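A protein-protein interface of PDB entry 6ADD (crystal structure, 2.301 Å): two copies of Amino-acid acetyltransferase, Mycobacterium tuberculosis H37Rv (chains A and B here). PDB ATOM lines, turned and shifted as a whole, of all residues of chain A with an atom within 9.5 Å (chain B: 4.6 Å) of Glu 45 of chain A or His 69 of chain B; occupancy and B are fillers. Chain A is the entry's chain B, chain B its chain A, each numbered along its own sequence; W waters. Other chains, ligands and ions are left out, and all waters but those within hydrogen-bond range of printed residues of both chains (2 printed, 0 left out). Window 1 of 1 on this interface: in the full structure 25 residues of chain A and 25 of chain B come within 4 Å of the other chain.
4 positions are printed for both chains.
Water W1 lies within hydrogen-bond range of N of Val 70 of chain B (2.8 Å), O of Glu 45 of chain A (2.8 Å), OE1 of Glu 49 of chain B (2.8 Å), NE2 of Gln 48 of chain A (2.9 Å) and ND1 of His 69 of chain B (3.5 Å).
Water W2 lies within hydrogen-bond range of OE1 of Gln 48 of chain A and O of Glu 49 of chain B.
Hydrophobic or aromatic side chains of chain A within 4 Å of the printed part of chain B: Val 41 and Val 47.
Hydrophobic or aromatic side chains of chain B that line the printed part of chain A: His 69, Val 70 and Val 151.
The backbone NH of Asp 148 of chain B sits at hydrogen-bond distance from the side-chain hydroxyl of Ser 146 of chain B, 3.0 Å away.
OD1 of Asp 148 of chain B is in salt-bridge range of NH2 of Arg 79 of chain B, at 2.8 Å.
The backbone carbonyl oxygen (O) of His 69 of chain B lies within hydrogen-bond range of the backbone NH (N) of Glu 77 of chain B (2.7 Å).
The backbone NH of Leu 68 of chain B lies within hydrogen-bond range of the backbone carbonyl oxygen of Glu 49 of chain B, at 3.3 Å.
The side-chain carboxylate (OE2) of Glu 49 of chain B sits at hydrogen-bond distance from a ring nitrogen (ND1) of His 69 of chain B (2.8 Å).
The side-chain carboxylate of Asp 148 of chain B sits at hydrogen-bond distance from the backbone NH of Val 151 of chain B (2.8 Å).
The side-chain hydroxyl (OG) of Ser 146 of chain B sits at hydrogen-bond distance from the side-chain carboxylate (OE2) of Glu 45 of chain A (2.6 Å).
NE2 of Gln 48 of chain A lies within hydrogen-bond range of O of Leu 68 of chain B (3.0 Å).
A ring nitrogen (NE2) of His 69 of chain B sits at hydrogen-bond distance from the side-chain carboxylate (OE1) of Glu 45 of chain A (2.6 Å).
Among the printed residues, merely in contact across the chains: Tyr 44 of chain A with Val 70 of chain B (3.3 Å), Glu 45 of chain A with Val 70 of chain B (3.3 Å), Glu 45 of chain A with Asp 148 of chain B (3.4 Å), Gln 48 of chain A with Glu 49 of chain B (3.5 Å), Glu 45 of chain A with Val 151 of chain B (3.6 Å), Val 47 of chain A with Val 70 of chain B (3.7 Å), Val 41 of chain A with Ser 146 of chain B (3.7 Å), Gln 48 of chain A with Val 70 of chain B (3.8 Å), Glu 45 of chain A with Glu 49 of chain B (3.96 Å) and Val 41 of chain A with Leu 71 of chain B (3.9997 Å).
Leu 43 of chain A touches none of the printed residues of chain B.
Printed residues of chain B within 4 Å of Tyr 44 of chain A: Val 70.
Printed residues of chain B within 4 Å of Glu 45 of chain A: Glu 49, His 69, Val 70, Ser 146, Asp 148 and Val 151.
Ala 46 of chain A touches none of the printed residues of chain B.
Of the printed residues of chain B, Val 47 of chain A touches Val 70 (3.7 Å).
Of the printed residues of chain B, Gln 48 of chain A touches Glu 49 (3.5 Å), Leu 68 (3.0 Å) and Val 70 (3.8 Å).
Of the printed residues of chain A, Glu 49 of chain B touches Glu 45 and Gln 48.
Leu 68 of chain B touches one residue of chain A.
His 69 of chain B touches just one residue of chain A: Glu 45.
Val 70 of chain B touches just these residues of chain A: Tyr 44 (3.3 Å), Glu 45 (3.3 Å), Val 47 (3.7 Å) and Gln 48 (3.8 Å).
No residue of chain A comes within 4 Å of Gly 76 of chain B.
Of the printed residues of chain A, Ser 146 of chain B touches Val 41 (3.7 Å) and Glu 45 (2.6 Å).
The nearest residue of chain A that does not touch His 69 of chain B is Gln 48 of chain A (4.6 Å).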
ATOM      1  N   THR A  17     -22.874 -27.393  17.923  1.00  0.00           N
ATOM      2  CA  THR A  17     -21.619 -28.038  18.315  1.00  0.00           C
ATOM      3  C   THR A  17     -20.719 -28.293  17.111  1.00  0.00           C
ATOM      4  O   THR A  17     -19.498 -28.365  17.266  1.00  0.00           O
ATOM      5  CB  THR A  17     -21.862 -29.359  19.060  1.00  0.00           C
ATOM      6  OG1 THR A  17     -22.594 -30.264  18.221  1.00  0.00           O
ATOM      7  CG2 THR A  17     -22.618 -29.124  20.372  1.00  0.00           C
ATOM      8  N   VAL A  20     -18.111 -25.554  16.603  1.00  0.00           N
ATOM      9  CA  VAL A  20     -17.067 -25.278  17.600  1.00  0.00           C
ATOM     10  C   VAL A  20     -15.657 -25.340  17.009  1.00  0.00           C
ATOM     11  O   VAL A  20     -14.841 -24.459  17.328  1.00  0.00           O
ATOM     12  CB  VAL A  20     -17.258 -26.170  18.833  1.00  0.00           C
ATOM     13  CG1 VAL A  20     -15.993 -26.190  19.723  1.00  0.00           C
ATOM     14  CG2 VAL A  20     -18.450 -25.658  19.659  1.00  0.00           C
ATOM     15  N   LYS A  38      -9.450 -19.635  24.535  1.00  0.00           N
ATOM     16  CA  LYS A  38     -10.558 -20.540  24.811  1.00  0.00           C
ATOM     17  C   LYS A  38     -10.153 -21.923  24.331  1.00  0.00           C
ATOM     18  O   LYS A  38      -9.807 -22.097  23.161  1.00  0.00           O
ATOM     19  CB  LYS A  38     -11.857 -20.071  24.143  1.00  0.00           C
ATOM     20  CG  LYS A  38     -12.481 -18.836  24.802  1.00  0.00           C
ATOM     21  CD  LYS A  38     -12.773 -19.091  26.277  1.00  0.00           C
ATOM     22  CE  LYS A  38     -13.593 -17.977  26.909  1.00  0.00           C
ATOM     23  NZ  LYS A  38     -12.966 -16.660  26.725  1.00  0.00           N
ATOM     24  N   ASN A  39     -10.100 -22.883  25.243  1.00  0.00           N
ATOM     25  CA  ASN A  39      -9.821 -24.229  24.778  1.00  0.00           C
ATOM     26  C   ASN A  39     -11.114 -24.893  24.308  1.00  0.00           C
ATOM     27  O   ASN A  39     -12.217 -24.352  24.462  1.00  0.00           O
ATOM     28  CB  ASN A  39      -9.122 -25.045  25.860  1.00  0.00           C
ATOM     29  CG  ASN A  39      -9.835 -24.994  27.183  1.00  0.00           C
ATOM     30  OD1 ASN A  39     -11.047 -25.197  27.250  1.00  0.00           O
ATOM     31  ND2 ASN A  39      -9.086 -24.718  28.253  1.00  0.00           N
ATOM     32  N   LEU A  40     -10.971 -26.076  23.697  1.00  0.00           N
ATOM     33  CA  LEU A  40     -12.115 -26.701  23.041  1.00  0.00           C
ATOM     34  C   LEU A  40     -13.241 -26.990  24.035  1.00  0.00           C
ATOM     35  O   LEU A  40     -14.421 -26.770  23.730  1.00  0.00           O
ATOM     36  CB  LEU A  40     -11.688 -27.973  22.301  1.00  0.00           C
ATOM     37  CG  LEU A  40     -11.086 -27.806  20.892  1.00  0.00           C
ATOM     38  CD1 LEU A  40     -10.588 -29.159  20.306  1.00  0.00           C
ATOM     39  CD2 LEU A  40     -12.069 -27.154  19.930  1.00  0.00           C
ATOM     40  N   VAL A  41     -12.905 -27.522  25.212  1.00  0.00           N
ATOM     41  CA  VAL A  41     -13.967 -27.937  26.131  1.00  0.00           C
ATOM     42  C   VAL A  41     -14.794 -26.739  26.575  1.00  0.00           C
ATOM     43  O   VAL A  41     -16.025 -26.806  26.645  1.00  0.00           O
ATOM     44  CB  VAL A  41     -13.390 -28.722  27.327  1.00  0.00           C
ATOM     45  CG1 VAL A  41     -12.493 -27.841  28.213  1.00  0.00           C
ATOM     46  CG2 VAL A  41     -14.522 -29.298  28.144  1.00  0.00           C
ATOM     47  N   THR A  42     -14.131 -25.616  26.833  1.00  0.00           N
ATOM     48  CA  THR A  42     -14.807 -24.389  27.244  1.00  0.00           C
ATOM     49  C   THR A  42     -15.750 -23.899  26.160  1.00  0.00           C
ATOM     50  O   THR A  42     -16.840 -23.389  26.451  1.00  0.00           O
ATOM     51  CB  THR A  42     -13.743 -23.342  27.580  1.00  0.00           C
ATOM     52  OG1 THR A  42     -12.938 -23.845  28.654  1.00  0.00           O
ATOM     53  CG2 THR A  42     -14.366 -22.015  27.974  1.00  0.00           C
ATOM     54  N   LEU A  43     -15.343 -24.042  24.901  1.00  0.00           N
ATOM     55  CA  LEU A  43     -16.220 -23.657  23.802  1.00  0.00           C
ATOM     56  C   LEU A  43     -17.431 -24.583  23.698  1.00  0.00           C
ATOM     57  O   LEU A  43     -18.552 -24.113  23.442  1.00  0.00           O
ATOM     58  CB  LEU A  43     -15.435 -23.639  22.494  1.00  0.00           C
ATOM     59  CG  LEU A  43     -14.389 -22.534  22.421  1.00  0.00           C
ATOM     60  CD1 LEU A  43     -13.622 -22.687  21.134  1.00  0.00           C
ATOM     61  CD2 LEU A  43     -15.059 -21.160  22.499  1.00  0.00           C
ATOM     62  N   TYR A  44     -17.241 -25.903  23.883  1.00  0.00           N
ATOM     63  CA  TYR A  44     -18.408 -26.782  23.890  1.00  0.00           C
ATOM     64  C   TYR A  44     -19.334 -26.418  25.039  1.00  0.00           C
ATOM     65  O   TYR A  44     -20.550 -26.295  24.847  1.00  0.00           O
ATOM     66  CB  TYR A  44     -17.991 -28.249  23.971  1.00  0.00           C
ATOM     67  CG  TYR A  44     -17.486 -28.776  22.647  1.00  0.00           C
ATOM     68  CD1 TYR A  44     -18.344 -28.914  21.547  1.00  0.00           C
ATOM     69  CD2 TYR A  44     -16.145 -29.092  22.479  1.00  0.00           C
ATOM     70  CE1 TYR A  44     -17.874 -29.361  20.323  1.00  0.00           C
ATOM     71  CE2 TYR A  44     -15.668 -29.541  21.264  1.00  0.00           C
ATOM     72  CZ  TYR A  44     -16.537 -29.686  20.198  1.00  0.00           C
ATOM     73  OH  TYR A  44     -16.047 -30.134  19.008  1.00  0.00           O
ATOM     74  N   GLU A  45     -18.763 -26.183  26.227  1.00  0.00           N
ATOM     75  CA  GLU A  45     -19.565 -25.824  27.391  1.00  0.00           C
ATOM     76  C   GLU A  45     -20.338 -24.533  27.172  1.00  0.00           C
ATOM     77  O   GLU A  45     -21.423 -24.359  27.744  1.00  0.00           O
ATOM     78  CB  GLU A  45     -18.675 -25.690  28.626  1.00  0.00           C
ATOM     79  CG  GLU A  45     -18.018 -27.000  29.059  1.00  0.00           C
ATOM     80  CD  GLU A  45     -17.278 -26.875  30.374  1.00  0.00           C
ATOM     81  OE1 GLU A  45     -17.937 -26.825  31.436  1.00  0.00           O
ATOM     82  OE2 GLU A  45     -16.029 -26.809  30.350  1.00  0.00           O
ATOM     83  N   ALA A  46     -19.811 -23.618  26.354  1.00  0.00           N
ATOM     84  CA  ALA A  46     -20.437 -22.314  26.173  1.00  0.00           C
ATOM     85  C   ALA A  46     -21.262 -22.220  24.897  1.00  0.00           C
ATOM     86  O   ALA A  46     -21.684 -21.126  24.534  1.00  0.00           O
ATOM     87  CB  ALA A  46     -19.377 -21.205  26.192  1.00  0.00           C
ATOM     88  N   VAL A  47     -21.560 -23.348  24.249  1.00  0.00           N
ATOM     89  CA  VAL A  47     -22.147 -23.302  22.911  1.00  0.00           C
ATOM     90  C   VAL A  47     -23.558 -22.714  22.929  1.00  0.00           C
ATOM     91  O   VAL A  47     -23.999 -22.119  21.936  1.00  0.00           O
ATOM     92  CB  VAL A  47     -22.113 -24.715  22.286  1.00  0.00           C
ATOM     93  CG1 VAL A  47     -23.138 -25.631  22.969  1.00  0.00           C
ATOM     94  CG2 VAL A  47     -22.343 -24.659  20.771  1.00  0.00           C
ATOM     95  N   GLN A  48     -24.276 -22.828  24.050  1.00  0.00           N
ATOM     96  CA  GLN A  48     -25.635 -22.295  24.142  1.00  0.00           C
ATOM     97  C   GLN A  48     -25.669 -20.784  24.345  1.00  0.00           C
ATOM     98  O   GLN A  48     -26.754 -20.207  24.473  1.00  0.00           O
ATOM     99  CB  GLN A  48     -26.393 -23.002  25.266  1.00  0.00           C
ATOM    100  CG  GLN A  48     -26.403 -24.509  25.051  1.00  0.00           C
ATOM    101  CD  GLN A  48     -27.069 -25.279  26.157  1.00  0.00           C
ATOM    102  OE1 GLN A  48     -28.298 -25.408  26.178  1.00  0.00           O
ATOM    103  NE2 GLN A  48     -26.267 -25.847  27.055  1.00  0.00           N
ATOM    104  N   GLU A  49     -24.517 -20.126  24.357  1.00  0.00           N
ATOM    105  CA  GLU A  49     -24.483 -18.680  24.370  1.00  0.00           C
ATOM    106  C   GLU A  49     -23.686 -18.118  23.207  1.00  0.00           C
ATOM    107  O   GLU A  49     -23.573 -16.895  23.089  1.00  0.00           O
ATOM    108  CB  GLU A  49     -23.906 -18.170  25.701  1.00  0.00           C
ATOM    109  CG  GLU A  49     -22.408 -18.350  25.874  1.00  0.00           C
ATOM    110  CD  GLU A  49     -21.915 -17.841  27.220  1.00  0.00           C
ATOM    111  OE1 GLU A  49     -22.621 -18.061  28.231  1.00  0.00           O
ATOM    112  OE2 GLU A  49     -20.831 -17.211  27.267  1.00  0.00           O
ATOM    113  N   PHE A  50     -23.189 -18.960  22.314  1.00  0.00           N
ATOM    114  CA  PHE A  50     -22.405 -18.495  21.181  1.00  0.00           C
ATOM    115  C   PHE A  50     -23.279 -18.361  19.944  1.00  0.00           C
ATOM    116  O   PHE A  50     -24.217 -19.129  19.731  1.00  0.00           O
ATOM    117  CB  PHE A  50     -21.243 -19.448  20.884  1.00  0.00           C
ATOM    118  CG  PHE A  50     -19.923 -18.980  21.420  1.00  0.00           C
ATOM    119  CD1 PHE A  50     -19.080 -18.178  20.655  1.00  0.00           C
ATOM    120  CD2 PHE A  50     -19.527 -19.334  22.697  1.00  0.00           C
ATOM    121  CE1 PHE A  50     -17.867 -17.755  21.157  1.00  0.00           C
ATOM    122  CE2 PHE A  50     -18.311 -18.913  23.200  1.00  0.00           C
ATOM    123  CZ  PHE A  50     -17.485 -18.121  22.434  1.00  0.00           C
ATOM    124  N   HIS A  69     -22.343 -13.212  27.445  1.00  0.00           N
ATOM    125  CA  HIS A  69     -22.140 -13.889  28.721  1.00  0.00           C
ATOM    126  C   HIS A  69     -22.806 -13.065  29.816  1.00  0.00           C
ATOM    127  O   HIS A  69     -22.480 -11.890  29.993  1.00  0.00           O
ATOM    128  CB  HIS A  69     -20.648 -14.076  29.009  1.00  0.00           C
ATOM    129  CG  HIS A  69     -20.358 -15.057  30.099  1.00  0.00           C
ATOM    130  ND1 HIS A  69     -20.541 -16.415  29.947  1.00  0.00           N
ATOM    131  CD2 HIS A  69     -19.911 -14.880  31.364  1.00  0.00           C
ATOM    132  CE1 HIS A  69     -20.205 -17.034  31.066  1.00  0.00           C
ATOM    133  NE2 HIS A  69     -19.821 -16.125  31.941  1.00  0.00           N
ATOM    134  N   ARG A  79     -18.320 -10.860  24.402  1.00  0.00           N
ATOM    135  CA  ARG A  79     -16.994 -11.462  24.472  1.00  0.00           C
ATOM    136  C   ARG A  79     -16.752 -12.352  23.260  1.00  0.00           C
ATOM    137  O   ARG A  79     -17.691 -12.808  22.593  1.00  0.00           O
ATOM    138  CB  ARG A  79     -16.809 -12.283  25.759  1.00  0.00           C
ATOM    139  CG  ARG A  79     -17.874 -13.361  25.975  1.00  0.00           C
ATOM    140  CD  ARG A  79     -17.442 -14.490  26.959  1.00  0.00           C
ATOM    141  NE  ARG A  79     -17.191 -14.018  28.321  1.00  0.00           N
ATOM    142  CZ  ARG A  79     -16.881 -14.791  29.367  1.00  0.00           C
ATOM    143  NH1 ARG A  79     -16.777 -16.119  29.260  1.00  0.00           N
ATOM    144  NH2 ARG A  79     -16.679 -14.218  30.545  1.00  0.00           N
ATOM    145  N   TYR A 147     -15.473 -18.754  38.595  1.00  0.00           N
ATOM    146  CA  TYR A 147     -14.312 -19.436  38.035  1.00  0.00           C
ATOM    147  C   TYR A 147     -13.938 -18.939  36.645  1.00  0.00           C
ATOM    148  O   TYR A 147     -12.874 -19.304  36.137  1.00  0.00           O
ATOM    149  CB  TYR A 147     -14.567 -20.951  37.954  1.00  0.00           C
ATOM    150  CG  TYR A 147     -14.940 -21.593  39.272  1.00  0.00           C
ATOM    151  CD1 TYR A 147     -13.959 -22.085  40.130  1.00  0.00           C
ATOM    152  CD2 TYR A 147     -16.270 -21.706  39.662  1.00  0.00           C
ATOM    153  CE1 TYR A 147     -14.294 -22.670  41.340  1.00  0.00           C
ATOM    154  CE2 TYR A 147     -16.614 -22.286  40.871  1.00  0.00           C
ATOM    155  CZ  TYR A 147     -15.622 -22.769  41.703  1.00  0.00           C
ATOM    156  OH  TYR A 147     -15.959 -23.347  42.905  1.00  0.00           O
ATOM    157  N   ASP A 148     -14.773 -18.108  36.030  1.00  0.00           N
ATOM    158  CA  ASP A 148     -14.555 -17.666  34.659  1.00  0.00           C
ATOM    159  C   ASP A 148     -13.522 -16.538  34.623  1.00  0.00           C
ATOM    160  O   ASP A 148     -13.641 -15.551  35.349  1.00  0.00           O
ATOM    161  CB  ASP A 148     -15.893 -17.223  34.062  1.00  0.00           C
ATOM    162  CG  ASP A 148     -15.775 -16.737  32.644  1.00  0.00           C
ATOM    163  OD1 ASP A 148     -15.311 -15.607  32.452  1.00  0.00           O
ATOM    164  OD2 ASP A 148     -16.179 -17.474  31.716  1.00  0.00           O
ATOM    165  N   GLU B  49     -28.588 -21.838  29.963  1.00  0.00           N
ATOM    166  CA  GLU B  49     -28.745 -23.275  29.837  1.00  0.00           C
ATOM    167  C   GLU B  49     -29.643 -23.857  30.919  1.00  0.00           C
ATOM    168  O   GLU B  49     -29.783 -25.087  30.993  1.00  0.00           O
ATOM    169  CB  GLU B  49     -27.373 -23.971  29.843  1.00  0.00           C
ATOM    170  CG  GLU B  49     -26.687 -23.951  31.175  1.00  0.00           C
ATOM    171  CD  GLU B  49     -25.306 -24.575  31.122  1.00  0.00           C
ATOM    172  OE1 GLU B  49     -24.558 -24.277  30.169  1.00  0.00           O
ATOM    173  OE2 GLU B  49     -24.986 -25.388  32.028  1.00  0.00           O
ATOM    174  N   ALA B  67     -30.609 -28.009  34.424  1.00  0.00           N
ATOM    175  CA  ALA B  67     -29.767 -27.496  33.355  1.00  0.00           C
ATOM    176  C   ALA B  67     -29.273 -28.642  32.486  1.00  0.00           C
ATOM    177  O   ALA B  67     -29.101 -29.771  32.956  1.00  0.00           O
ATOM    178  CB  ALA B  67     -28.545 -26.712  33.916  1.00  0.00           C
ATOM    179  N   LEU B  68     -29.070 -28.343  31.206  1.00  0.00           N
ATOM    180  CA  LEU B  68     -28.386 -29.233  30.272  1.00  0.00           C
ATOM    181  C   LEU B  68     -27.043 -28.588  29.954  1.00  0.00           C
ATOM    182  O   LEU B  68     -26.996 -27.474  29.421  1.00  0.00           O
ATOM    183  CB  LEU B  68     -29.204 -29.456  29.003  1.00  0.00           C
ATOM    184  CG  LEU B  68     -28.782 -30.553  28.013  1.00  0.00           C
ATOM    185  CD1 LEU B  68     -27.636 -30.105  27.104  1.00  0.00           C
ATOM    186  CD2 LEU B  68     -28.418 -31.854  28.744  1.00  0.00           C
ATOM    187  N   HIS B  69     -25.964 -29.269  30.318  1.00  0.00           N
ATOM    188  CA  HIS B  69     -24.605 -28.760  30.175  1.00  0.00           C
ATOM    189  C   HIS B  69     -23.878 -29.549  29.090  1.00  0.00           C
ATOM    190  O   HIS B  69     -23.746 -30.775  29.192  1.00  0.00           O
ATOM    191  CB  HIS B  69     -23.850 -28.851  31.503  1.00  0.00           C
ATOM    192  CG  HIS B  69     -22.565 -28.075  31.520  1.00  0.00           C
ATOM    193  ND1 HIS B  69     -22.530 -26.698  31.489  1.00  0.00           N
ATOM    194  CD2 HIS B  69     -21.272 -28.482  31.558  1.00  0.00           C
ATOM    195  CE1 HIS B  69     -21.274 -26.286  31.512  1.00  0.00           C
ATOM    196  NE2 HIS B  69     -20.489 -27.349  31.561  1.00  0.00           N
ATOM    197  N   VAL B  70     -23.401 -28.853  28.063  1.00  0.00           N
ATOM    198  CA  VAL B  70     -22.667 -29.504  26.981  1.00  0.00           C
ATOM    199  C   VAL B  70     -21.248 -29.811  27.437  1.00  0.00           C
ATOM    200  O   VAL B  70     -20.552 -28.939  27.972  1.00  0.00           O
ATOM    201  CB  VAL B  70     -22.673 -28.635  25.716  1.00  0.00           C
ATOM    202  CG1 VAL B  70     -21.860 -29.307  24.612  1.00  0.00           C
ATOM    203  CG2 VAL B  70     -24.112 -28.381  25.270  1.00  0.00           C
ATOM    204  N   LEU B  71     -20.820 -31.062  27.229  1.00  0.00           N
ATOM    205  CA  LEU B  71     -19.491 -31.543  27.585  1.00  0.00           C
ATOM    206  C   LEU B  71     -18.572 -31.733  26.396  1.00  0.00           C
ATOM    207  O   LEU B  71     -17.355 -31.627  26.548  1.00  0.00           O
ATOM    208  CB  LEU B  71     -19.585 -32.886  28.323  1.00  0.00           C
ATOM    209  CG  LEU B  71     -20.387 -32.945  29.623  1.00  0.00           C
ATOM    210  CD1 LEU B  71     -20.434 -34.388  30.160  1.00  0.00           C
ATOM    211  CD2 LEU B  71     -19.799 -32.011  30.661  1.00  0.00           C
ATOM    212  N   GLY B  76     -23.613 -34.525  26.380  1.00  0.00           N
ATOM    213  CA  GLY B  76     -24.126 -33.546  27.306  1.00  0.00           C
ATOM    214  C   GLY B  76     -24.382 -34.173  28.666  1.00  0.00           C
ATOM    215  O   GLY B  76     -24.329 -35.394  28.837  1.00  0.00           O
ATOM    216  N   GLU B  77     -24.680 -33.311  29.629  1.00  0.00           N
ATOM    217  CA  GLU B  77     -24.926 -33.745  30.989  1.00  0.00           C
ATOM    218  C   GLU B  77     -26.169 -33.054  31.516  1.00  0.00           C
ATOM    219  O   GLU B  77     -26.357 -31.847  31.317  1.00  0.00           O
ATOM    220  CB  GLU B  77     -23.724 -33.440  31.876  1.00  0.00           C
ATOM    221  CG  GLU B  77     -24.074 -33.386  33.324  1.00  0.00           C
ATOM    222  CD  GLU B  77     -22.884 -33.102  34.199  1.00  0.00           C
ATOM    223  OE1 GLU B  77     -22.473 -31.933  34.311  1.00  0.00           O
ATOM    224  OE2 GLU B  77     -22.365 -34.062  34.782  1.00  0.00           O
ATOM    225  N   ARG B  79     -27.714 -31.755  34.837  1.00  0.00           N
ATOM    226  CA  ARG B  79     -27.153 -31.365  36.123  1.00  0.00           C
ATOM    227  C   ARG B  79     -28.105 -30.395  36.807  1.00  0.00           C
ATOM    228  O   ARG B  79     -28.920 -29.725  36.161  1.00  0.00           O
ATOM    229  CB  ARG B  79     -25.758 -30.720  35.968  1.00  0.00           C
ATOM    230  CG  ARG B  79     -25.761 -29.463  35.072  1.00  0.00           C
ATOM    231  CD  ARG B  79     -24.532 -28.601  35.238  1.00  0.00           C
ATOM    232  NE  ARG B  79     -23.297 -29.303  34.873  1.00  0.00           N
ATOM    233  CZ  ARG B  79     -22.077 -28.755  34.895  1.00  0.00           C
ATOM    234  NH1 ARG B  79     -21.908 -27.470  35.257  1.00  0.00           N
ATOM    235  NH2 ARG B  79     -21.020 -29.503  34.567  1.00  0.00           N
ATOM    236  N   SER B 146     -10.986 -28.023  31.610  1.00  0.00           N
ATOM    237  CA  SER B 146     -12.168 -27.299  32.051  1.00  0.00           C
ATOM    238  C   SER B 146     -12.016 -26.808  33.485  1.00  0.00           C
ATOM    239  O   SER B 146     -11.441 -27.480  34.338  1.00  0.00           O
ATOM    240  CB  SER B 146     -13.411 -28.189  31.950  1.00  0.00           C
ATOM    241  OG  SER B 146     -14.553 -27.487  32.405  1.00  0.00           O
ATOM    242  N   ASP B 148     -14.774 -26.287  35.188  1.00  0.00           N
ATOM    243  CA  ASP B 148     -16.037 -26.675  35.792  1.00  0.00           C
ATOM    244  C   ASP B 148     -15.872 -27.907  36.677  1.00  0.00           C
ATOM    245  O   ASP B 148     -15.329 -28.925  36.241  1.00  0.00           O
ATOM    246  CB  ASP B 148     -17.064 -26.929  34.695  1.00  0.00           C
ATOM    247  CG  ASP B 148     -18.393 -27.282  35.249  1.00  0.00           C
ATOM    248  OD1 ASP B 148     -18.583 -28.461  35.606  1.00  0.00           O
ATOM    249  OD2 ASP B 148     -19.227 -26.366  35.377  1.00  0.00           O
ATOM    250  N   VAL B 151     -17.545 -31.094  35.497  1.00  0.00           N
ATOM    251  CA  VAL B 151     -16.765 -31.803  34.485  1.00  0.00           C
ATOM    252  C   VAL B 151     -15.748 -32.732  35.142  1.00  0.00           C
ATOM    253  O   VAL B 151     -15.560 -33.880  34.712  1.00  0.00           O
ATOM    254  CB  VAL B 151     -16.093 -30.798  33.537  1.00  0.00           C
ATOM    255  CG1 VAL B 151     -15.156 -31.521  32.586  1.00  0.00           C
ATOM    256  CG2 VAL B 151     -17.147 -30.034  32.759  1.00  0.00           C
HETATM  257  O   HOH W   1     -23.602 -26.085  28.217  1.00  0.00           O
HETATM  258  O   HOH W   2     -30.466 -25.817  27.990  1.00  0.00           O
